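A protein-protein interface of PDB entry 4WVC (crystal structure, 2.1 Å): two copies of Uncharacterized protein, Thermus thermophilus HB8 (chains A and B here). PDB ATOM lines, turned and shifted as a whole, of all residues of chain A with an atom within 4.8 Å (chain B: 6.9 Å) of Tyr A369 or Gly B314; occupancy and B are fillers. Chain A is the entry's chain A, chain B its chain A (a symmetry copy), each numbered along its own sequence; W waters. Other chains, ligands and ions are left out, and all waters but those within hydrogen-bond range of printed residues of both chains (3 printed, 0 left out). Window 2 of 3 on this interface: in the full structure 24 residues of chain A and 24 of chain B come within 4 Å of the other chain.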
ATOM      1  N   LEU A 306      -7.956 -14.320  17.904  1.00  0.00           N
ATOM      2  CA  LEU A 306      -9.295 -14.523  17.325  1.00  0.00           C
ATOM      3  C   LEU A 306     -10.349 -13.947  18.266  1.00  0.00           C
ATOM      4  O   LEU A 306     -11.332 -13.372  17.821  1.00  0.00           O
ATOM      5  CB  LEU A 306      -9.562 -16.006  17.058  1.00  0.00           C
ATOM      6  CG  LEU A 306      -8.644 -16.659  16.010  1.00  0.00           C
ATOM      7  CD1 LEU A 306      -8.612 -18.155  16.200  1.00  0.00           C
ATOM      8  CD2 LEU A 306      -9.023 -16.322  14.576  1.00  0.00           C
ATOM      9  N   GLY A 309     -10.335 -10.223  17.715  1.00  0.00           N
ATOM     10  CA  GLY A 309     -10.887  -9.836  16.451  1.00  0.00           C
ATOM     11  C   GLY A 309      -9.950  -9.065  15.540  1.00  0.00           C
ATOM     12  O   GLY A 309     -10.427  -8.436  14.605  1.00  0.00           O
ATOM     13  N   THR A 310      -8.641  -9.116  15.780  1.00  0.00           N
ATOM     14  CA  THR A 310      -7.682  -8.413  14.920  1.00  0.00           C
ATOM     15  C   THR A 310      -7.239  -9.114  13.628  1.00  0.00           C
ATOM     16  O   THR A 310      -6.941  -8.439  12.631  1.00  0.00           O
ATOM     17  CB  THR A 310      -6.414  -7.997  15.692  1.00  0.00           C
ATOM     18  OG1 THR A 310      -5.731  -9.157  16.221  1.00  0.00           O
ATOM     19  CG2 THR A 310      -6.770  -7.092  16.797  1.00  0.00           C
ATOM     20  N   PRO A 311      -7.165 -10.456  13.625  1.00  0.00           N
ATOM     21  CA  PRO A 311      -6.682 -11.079  12.391  1.00  0.00           C
ATOM     22  C   PRO A 311      -7.598 -10.886  11.193  1.00  0.00           C
ATOM     23  O   PRO A 311      -8.812 -10.795  11.360  1.00  0.00           O
ATOM     24  CB  PRO A 311      -6.634 -12.581  12.738  1.00  0.00           C
ATOM     25  CG  PRO A 311      -6.842 -12.703  14.188  1.00  0.00           C
ATOM     26  CD  PRO A 311      -7.307 -11.412  14.735  1.00  0.00           C
ATOM     27  N   HIS A 312      -7.034 -10.854   9.994  1.00  0.00           N
ATOM     28  CA  HIS A 312      -7.864 -11.057   8.789  1.00  0.00           C
ATOM     29  C   HIS A 312      -8.241 -12.555   8.634  1.00  0.00           C
ATOM     30  O   HIS A 312      -7.694 -13.411   9.327  1.00  0.00           O
ATOM     31  CB  HIS A 312      -7.230 -10.452   7.506  1.00  0.00           C
ATOM     32  CG  HIS A 312      -5.879 -10.988   7.138  1.00  0.00           C
ATOM     33  ND1 HIS A 312      -5.679 -12.278   6.698  1.00  0.00           N
ATOM     34  CD2 HIS A 312      -4.679 -10.365   7.026  1.00  0.00           C
ATOM     35  CE1 HIS A 312      -4.406 -12.444   6.397  1.00  0.00           C
ATOM     36  NE2 HIS A 312      -3.783 -11.290   6.552  1.00  0.00           N
ATOM     37  N   GLN A 313      -9.180 -12.859   7.743  1.00  0.00           N
ATOM     38  CA  GLN A 313      -9.713 -14.223   7.580  1.00  0.00           C
ATOM     39  C   GLN A 313      -8.672 -15.290   7.218  1.00  0.00           C
ATOM     40  O   GLN A 313      -8.835 -16.444   7.557  1.00  0.00           O
ATOM     41  CB  GLN A 313     -10.734 -14.192   6.462  1.00  0.00           C
ATOM     42  CG  GLN A 313     -11.478 -15.499   6.195  1.00  0.00           C
ATOM     43  CD  GLN A 313     -12.388 -15.831   7.322  1.00  0.00           C
ATOM     44  OE1 GLN A 313     -12.637 -14.996   8.184  1.00  0.00           O
ATOM     45  NE2 GLN A 313     -12.900 -17.040   7.329  1.00  0.00           N
ATOM     46  N   ALA A 316      -6.914 -16.298  10.334  1.00  0.00           N
ATOM     47  CA  ALA A 316      -7.847 -17.155  11.044  1.00  0.00           C
ATOM     48  C   ALA A 316      -7.883 -18.539  10.412  1.00  0.00           C
ATOM     49  O   ALA A 316      -7.951 -19.538  11.122  1.00  0.00           O
ATOM     50  CB  ALA A 316      -9.234 -16.547  11.053  1.00  0.00           C
ATOM     51  N   GLY A 365     -14.027 -16.798  19.348  1.00  0.00           N
ATOM     52  CA  GLY A 365     -13.175 -16.290  18.278  1.00  0.00           C
ATOM     53  C   GLY A 365     -13.361 -16.925  16.910  1.00  0.00           C
ATOM     54  O   GLY A 365     -13.500 -16.218  15.913  1.00  0.00           O
ATOM     55  N   PHE A 366     -13.361 -18.250  16.846  1.00  0.00           N
ATOM     56  CA  PHE A 366     -13.561 -18.949  15.571  1.00  0.00           C
ATOM     57  C   PHE A 366     -14.967 -18.754  15.019  1.00  0.00           C
ATOM     58  O   PHE A 366     -15.157 -18.644  13.818  1.00  0.00           O
ATOM     59  CB  PHE A 366     -13.291 -20.449  15.728  1.00  0.00           C
ATOM     60  CG  PHE A 366     -11.856 -20.816  15.569  1.00  0.00           C
ATOM     61  CD1 PHE A 366     -11.190 -20.525  14.385  1.00  0.00           C
ATOM     62  CD2 PHE A 366     -11.174 -21.464  16.581  1.00  0.00           C
ATOM     63  CE1 PHE A 366      -9.870 -20.865  14.220  1.00  0.00           C
ATOM     64  CE2 PHE A 366      -9.850 -21.801  16.429  1.00  0.00           C
ATOM     65  CZ  PHE A 366      -9.198 -21.515  15.243  1.00  0.00           C
ATOM     66  N   ARG A 367     -15.942 -18.690  15.904  1.00  0.00           N
ATOM     67  CA  ARG A 367     -17.315 -18.432  15.499  1.00  0.00           C
ATOM     68  C   ARG A 367     -17.361 -17.099  14.725  1.00  0.00           C
ATOM     69  O   ARG A 367     -17.949 -17.019  13.649  1.00  0.00           O
ATOM     70  CB  ARG A 367     -18.226 -18.409  16.736  1.00  0.00           C
ATOM     71  CG  ARG A 367     -19.713 -18.510  16.478  1.00  0.00           C
ATOM     72  CD  ARG A 367     -20.547 -18.244  17.753  1.00  0.00           C
ATOM     73  NE  ARG A 367     -19.874 -18.524  19.055  1.00  0.00           N
ATOM     74  CZ  ARG A 367     -19.757 -19.734  19.646  1.00  0.00           C
ATOM     75  NH1 ARG A 367     -20.236 -20.835  19.069  1.00  0.00           N
ATOM     76  NH2 ARG A 367     -19.148 -19.851  20.831  1.00  0.00           N
ATOM     77  N   ASP A 368     -16.683 -16.094  15.250  1.00  0.00           N
ATOM     78  CA  ASP A 368     -16.706 -14.736  14.700  1.00  0.00           C
ATOM     79  C   ASP A 368     -16.140 -14.691  13.293  1.00  0.00           C
ATOM     80  O   ASP A 368     -16.480 -13.815  12.491  1.00  0.00           O
ATOM     81  CB  ASP A 368     -15.857 -13.813  15.599  1.00  0.00           C
ATOM     82  CG  ASP A 368     -16.413 -13.673  16.992  1.00  0.00           C
ATOM     83  OD1 ASP A 368     -17.615 -14.018  17.188  1.00  0.00           O
ATOM     84  OD2 ASP A 368     -15.641 -13.239  17.898  1.00  0.00           O
ATOM     85  N   TYR A 369     -15.226 -15.614  13.021  1.00  0.00           N
ATOM     86  CA  TYR A 369     -14.553 -15.720  11.728  1.00  0.00           C
ATOM     87  C   TYR A 369     -15.153 -16.752  10.795  1.00  0.00           C
ATOM     88  O   TYR A 369     -14.597 -16.995   9.743  1.00  0.00           O
ATOM     89  CB  TYR A 369     -13.039 -15.996  11.925  1.00  0.00           C
ATOM     90  CG  TYR A 369     -12.273 -14.762  12.313  1.00  0.00           C
ATOM     91  CD1 TYR A 369     -12.209 -14.356  13.648  1.00  0.00           C
ATOM     92  CD2 TYR A 369     -11.651 -13.966  11.353  1.00  0.00           C
ATOM     93  CE1 TYR A 369     -11.541 -13.210  14.018  1.00  0.00           C
ATOM     94  CE2 TYR A 369     -10.964 -12.821  11.725  1.00  0.00           C
ATOM     95  CZ  TYR A 369     -10.906 -12.458  13.063  1.00  0.00           C
ATOM     96  OH  TYR A 369     -10.242 -11.341  13.491  1.00  0.00           O
ATOM     97  N   GLY A 370     -16.294 -17.343  11.168  1.00  0.00           N
ATOM     98  CA  GLY A 370     -17.058 -18.194  10.283  1.00  0.00           C
ATOM     99  C   GLY A 370     -16.728 -19.661  10.417  1.00  0.00           C
ATOM    100  O   GLY A 370     -17.205 -20.474   9.641  1.00  0.00           O
ATOM    101  N   PHE A 371     -15.900 -20.021  11.380  1.00  0.00           N
ATOM    102  CA  PHE A 371     -15.502 -21.415  11.529  1.00  0.00           C
ATOM    103  C   PHE A 371     -16.468 -22.081  12.510  1.00  0.00           C
ATOM    104  O   PHE A 371     -16.105 -22.395  13.648  1.00  0.00           O
ATOM    105  CB  PHE A 371     -14.036 -21.494  11.969  1.00  0.00           C
ATOM    106  CG  PHE A 371     -13.080 -21.039  10.907  1.00  0.00           C
ATOM    107  CD1 PHE A 371     -12.710 -21.895   9.898  1.00  0.00           C
ATOM    108  CD2 PHE A 371     -12.632 -19.744  10.873  1.00  0.00           C
ATOM    109  CE1 PHE A 371     -11.880 -21.478   8.874  1.00  0.00           C
ATOM    110  CE2 PHE A 371     -11.797 -19.313   9.868  1.00  0.00           C
ATOM    111  CZ  PHE A 371     -11.414 -20.185   8.864  1.00  0.00           C
ATOM    112  N   TRP B 277     -21.386  -4.344  16.057  1.00  0.00           N
ATOM    113  CA  TRP B 277     -21.596  -5.761  15.773  1.00  0.00           C
ATOM    114  C   TRP B 277     -21.965  -6.491  17.053  1.00  0.00           C
ATOM    115  O   TRP B 277     -21.284  -6.366  18.061  1.00  0.00           O
ATOM    116  CB  TRP B 277     -20.328  -6.370  15.163  1.00  0.00           C
ATOM    117  CG  TRP B 277     -20.425  -7.817  14.901  1.00  0.00           C
ATOM    118  CD1 TRP B 277     -19.950  -8.823  15.679  1.00  0.00           C
ATOM    119  CD2 TRP B 277     -21.047  -8.447  13.757  1.00  0.00           C
ATOM    120  NE1 TRP B 277     -20.235 -10.041  15.099  1.00  0.00           N
ATOM    121  CE2 TRP B 277     -20.900  -9.837  13.916  1.00  0.00           C
ATOM    122  CE3 TRP B 277     -21.698  -7.960  12.613  1.00  0.00           C
ATOM    123  CZ2 TRP B 277     -21.391 -10.754  12.978  1.00  0.00           C
ATOM    124  CZ3 TRP B 277     -22.193  -8.851  11.707  1.00  0.00           C
ATOM    125  CH2 TRP B 277     -22.031 -10.247  11.892  1.00  0.00           C
ATOM    126  N   PRO B 311     -15.920  -4.483   7.809  1.00  0.00           N
ATOM    127  CA  PRO B 311     -15.890  -5.842   8.354  1.00  0.00           C
ATOM    128  C   PRO B 311     -14.753  -6.702   7.827  1.00  0.00           C
ATOM    129  O   PRO B 311     -14.330  -6.525   6.687  1.00  0.00           O
ATOM    130  CB  PRO B 311     -17.227  -6.450   7.884  1.00  0.00           C
ATOM    131  CG  PRO B 311     -18.037  -5.356   7.329  1.00  0.00           C
ATOM    132  CD  PRO B 311     -17.195  -4.155   7.149  1.00  0.00           C
ATOM    133  N   HIS B 312     -14.279  -7.644   8.630  1.00  0.00           N
ATOM    134  CA  HIS B 312     -13.466  -8.743   8.070  1.00  0.00           C
ATOM    135  C   HIS B 312     -14.369  -9.757   7.318  1.00  0.00           C
ATOM    136  O   HIS B 312     -15.593  -9.701   7.423  1.00  0.00           O
ATOM    137  CB  HIS B 312     -12.542  -9.413   9.123  1.00  0.00           C
ATOM    138  CG  HIS B 312     -13.239 -10.013  10.306  1.00  0.00           C
ATOM    139  ND1 HIS B 312     -14.041 -11.130  10.216  1.00  0.00           N
ATOM    140  CD2 HIS B 312     -13.151  -9.724  11.629  1.00  0.00           C
ATOM    141  CE1 HIS B 312     -14.469 -11.459  11.420  1.00  0.00           C
ATOM    142  NE2 HIS B 312     -13.916 -10.645  12.300  1.00  0.00           N
ATOM    143  N   GLN B 313     -13.765 -10.665   6.557  1.00  0.00           N
ATOM    144  CA  GLN B 313     -14.505 -11.609   5.701  1.00  0.00           C
ATOM    145  C   GLN B 313     -15.491 -12.522   6.440  1.00  0.00           C
ATOM    146  O   GLN B 313     -16.484 -12.934   5.876  1.00  0.00           O
ATOM    147  CB  GLN B 313     -13.495 -12.502   5.011  1.00  0.00           C
ATOM    148  CG  GLN B 313     -14.057 -13.497   4.000  1.00  0.00           C
ATOM    149  CD  GLN B 313     -14.590 -12.794   2.804  1.00  0.00           C
ATOM    150  OE1 GLN B 313     -14.343 -11.607   2.622  1.00  0.00           O
ATOM    151  NE2 GLN B 313     -15.314 -13.509   1.974  1.00  0.00           N
ATOM    152  N   GLY B 314     -15.152 -12.870   7.680  1.00  0.00           N
ATOM    153  CA  GLY B 314     -15.978 -13.691   8.551  1.00  0.00           C
ATOM    154  C   GLY B 314     -17.290 -13.060   8.973  1.00  0.00           C
ATOM    155  O   GLY B 314     -18.309 -13.763   9.097  1.00  0.00           O
ATOM    156  N   ARG B 315     -17.279 -11.752   9.208  1.00  0.00           N
ATOM    157  CA  ARG B 315     -18.515 -11.030   9.455  1.00  0.00           C
ATOM    158  C   ARG B 315     -19.288 -10.860   8.182  1.00  0.00           C
ATOM    159  O   ARG B 315     -20.496 -10.966   8.192  1.00  0.00           O
ATOM    160  CB  ARG B 315     -18.277  -9.643  10.083  1.00  0.00           C
ATOM    161  CG  ARG B 315     -17.932  -9.782  11.531  1.00  0.00           C
ATOM    162  CD  ARG B 315     -17.878  -8.500  12.309  1.00  0.00           C
ATOM    163  NE  ARG B 315     -17.430  -8.805  13.667  1.00  0.00           N
ATOM    164  CZ  ARG B 315     -16.957  -7.925  14.527  1.00  0.00           C
ATOM    165  NH1 ARG B 315     -16.857  -6.635  14.210  1.00  0.00           N
ATOM    166  NH2 ARG B 315     -16.592  -8.341  15.726  1.00  0.00           N
ATOM    167  N   ALA B 316     -18.602 -10.591   7.082  1.00  0.00           N
ATOM    168  CA  ALA B 316     -19.292 -10.534   5.806  1.00  0.00           C
ATOM    169  C   ALA B 316     -19.973 -11.864   5.512  1.00  0.00           C
ATOM    170  O   ALA B 316     -21.088 -11.883   4.999  1.00  0.00           O
ATOM    171  CB  ALA B 316     -18.330 -10.180   4.690  1.00  0.00           C
ATOM    172  N   SER B 317     -19.277 -12.965   5.823  1.00  0.00           N
ATOM    173  CA  SER B 317     -19.793 -14.327   5.644  1.00  0.00           C
ATOM    174  C   SER B 317     -21.134 -14.518   6.365  1.00  0.00           C
ATOM    175  O   SER B 317     -22.117 -14.971   5.777  1.00  0.00           O
ATOM    176  CB  SER B 317     -18.773 -15.349   6.186  1.00  0.00           C
ATOM    177  OG  SER B 317     -18.626 -16.385   5.277  1.00  0.00           O
ATOM    178  N   LEU B 318     -21.129 -14.159   7.649  1.00  0.00           N
ATOM    179  CA  LEU B 318     -22.277 -14.268   8.513  1.00  0.00           C
ATOM    180  C   LEU B 318     -23.428 -13.407   8.012  1.00  0.00           C
ATOM    181  O   LEU B 318     -24.575 -13.818   8.073  1.00  0.00           O
ATOM    182  CB  LEU B 318     -21.883 -13.904   9.955  1.00  0.00           C
ATOM    183  CG  LEU B 318     -20.936 -14.917  10.614  1.00  0.00           C
ATOM    184  CD1 LEU B 318     -20.398 -14.424  11.955  1.00  0.00           C
ATOM    185  CD2 LEU B 318     -21.630 -16.259  10.783  1.00  0.00           C
ATOM    186  N   LEU B 319     -23.107 -12.232   7.490  1.00  0.00           N
ATOM    187  CA  LEU B 319     -24.114 -11.394   6.831  1.00  0.00           C
ATOM    188  C   LEU B 319     -24.623 -12.053   5.539  1.00  0.00           C
ATOM    189  O   LEU B 319     -25.822 -11.955   5.211  1.00  0.00           O
ATOM    190  CB  LEU B 319     -23.571  -9.983   6.555  1.00  0.00           C
ATOM    191  CG  LEU B 319     -23.442  -9.054   7.771  1.00  0.00           C
ATOM    192  CD1 LEU B 319     -22.779  -7.747   7.371  1.00  0.00           C
ATOM    193  CD2 LEU B 319     -24.806  -8.789   8.421  1.00  0.00           C
ATOM    194  N   GLN B 321     -24.850 -15.261   4.991  1.00  0.00           N
ATOM    195  CA  GLN B 321     -25.763 -16.276   5.486  1.00  0.00           C
ATOM    196  C   GLN B 321     -27.100 -15.674   5.944  1.00  0.00           C
ATOM    197  O   GLN B 321     -28.152 -16.238   5.674  1.00  0.00           O
ATOM    198  CB  GLN B 321     -25.112 -17.074   6.616  1.00  0.00           C
ATOM    199  CG  GLN B 321     -24.129 -18.119   6.118  1.00  0.00           C
ATOM    200  CD  GLN B 321     -22.980 -18.397   7.077  1.00  0.00           C
ATOM    201  OE1 GLN B 321     -23.163 -18.467   8.297  1.00  0.00           O
ATOM    202  NE2 GLN B 321     -21.779 -18.563   6.527  1.00  0.00           N
ATOM    203  N   TYR B 369     -16.506  -8.099  -1.054  1.00  0.00           N
ATOM    204  CA  TYR B 369     -16.124  -9.197  -0.168  1.00  0.00           C
ATOM    205  C   TYR B 369     -16.169 -10.566  -0.816  1.00  0.00           C
ATOM    206  O   TYR B 369     -15.979 -11.553  -0.133  1.00  0.00           O
ATOM    207  CB  TYR B 369     -16.996  -9.188   1.116  1.00  0.00           C
ATOM    208  CG  TYR B 369     -16.562  -8.137   2.100  1.00  0.00           C
ATOM    209  CD1 TYR B 369     -17.012  -6.821   1.979  1.00  0.00           C
ATOM    210  CD2 TYR B 369     -15.667  -8.435   3.126  1.00  0.00           C
ATOM    211  CE1 TYR B 369     -16.599  -5.838   2.850  1.00  0.00           C
ATOM    212  CE2 TYR B 369     -15.262  -7.450   4.014  1.00  0.00           C
ATOM    213  CZ  TYR B 369     -15.743  -6.157   3.873  1.00  0.00           C
ATOM    214  OH  TYR B 369     -15.382  -5.144   4.720  1.00  0.00           O
HETATM  215  O   HOH W   1     -19.448 -12.822  15.559  1.00  0.00           O
HETATM  216  O   HOH W   2     -17.489 -11.888  13.525  1.00  0.00           O
HETATM  217  O   HOH W   3     -16.988 -10.913  15.678  1.00  0.00           O
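The backbone carbonyl oxygen (O) of Pro A311 is in hydrogen-bond range of the side-chain hydroxyl (OH) of Tyr A369 (2.6 Å).
The backbone carbonyl oxygen of Tyr A369 lies within hydrogen-bond range of the side-chain amide nitrogen of Gln A313 (3.0 Å).
ND1 of His B312 lies within hydrogen-bond range of N of Arg B315.
N of Gly B314 sits close to ND1 of His B312, 3.3 Å away.
The side-chain amide nitrogen (NE2) of Gln B313 lies within hydrogen-bond range of the backbone carbonyl oxygen (O) of Tyr B369 (3.0 Å).
The backbone carbonyl oxygen of Gly A309 sits close to the side-chain hydroxyl of Tyr A369 (3.1 Å).
Gln B313 touches Gln A313 (CB to CB, 3.5 Å).
CD1 of Leu B318 touches O of Arg A367 (3.9 Å).
CE1 of His B312 touches O of Asp A368, 3.3 Å away.
Asp A368 touches Gly B314.
Arg B315 touches Asp A368 (N to O, 3.96 Å).
Tyr A369 touches His B312.
Gly B314 touches Tyr A369 (CA to O, 3.8 Å).
Gln A313 touches its own counterpart, Gln B313.
Tyr A369 touches His B312, but with the chains exchanged His A312 does not touch Tyr B369 (9.3 Å).
Water W2 bridges O of Asp A368 (2.4 Å) and NE of Arg B315 (3.1 Å).
Water W3 lies within hydrogen-bond range of NH2 of Arg B315 (2.6 Å), NE1 of Trp B277 (3.4 Å) and OD2 of Asp A368 (3.5 Å).
Water W1 bridges the side-chain carboxylate of Asp A368 and the indole nitrogen of Trp B277.
Tyr A369 touches just these residues of chain B: His B312 and Gly B314.
Pro B311 touches none of the printed residues of chain A.
Printed residues of chain A within 4 Å of Gln B313: Gln A313.
Gly B314 touches just these residues of chain A: Gln A313 (3.3 Å), Asp A368 (3.7 Å) and Tyr A369 (3.8 Å).
Of the printed residues of chain A, Arg B315 touches Asp A368.
The nearest printed residue of chain B that does not touch Tyr A369 is Leu B318 (5.4 Å).
The nearest residue of chain A that does not touch Gly B314 is Gly A370 (4.5 Å).
The nearest printed residue of chain B that does not touch Gln A313 is His B312 (4.6 Å).
Hydrophobic or aromatic side chains of chain B that line the printed part of chain A: His B312 and Leu B318.
Hydrophobic or aromatic side chains of chain A that line the printed part of chain B: Tyr A369.
The backbone NH (N) of Gly B314 is in hydrogen-bond range of the side-chain amide oxygen (OE1) of Gln A313 (3.3 Å).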
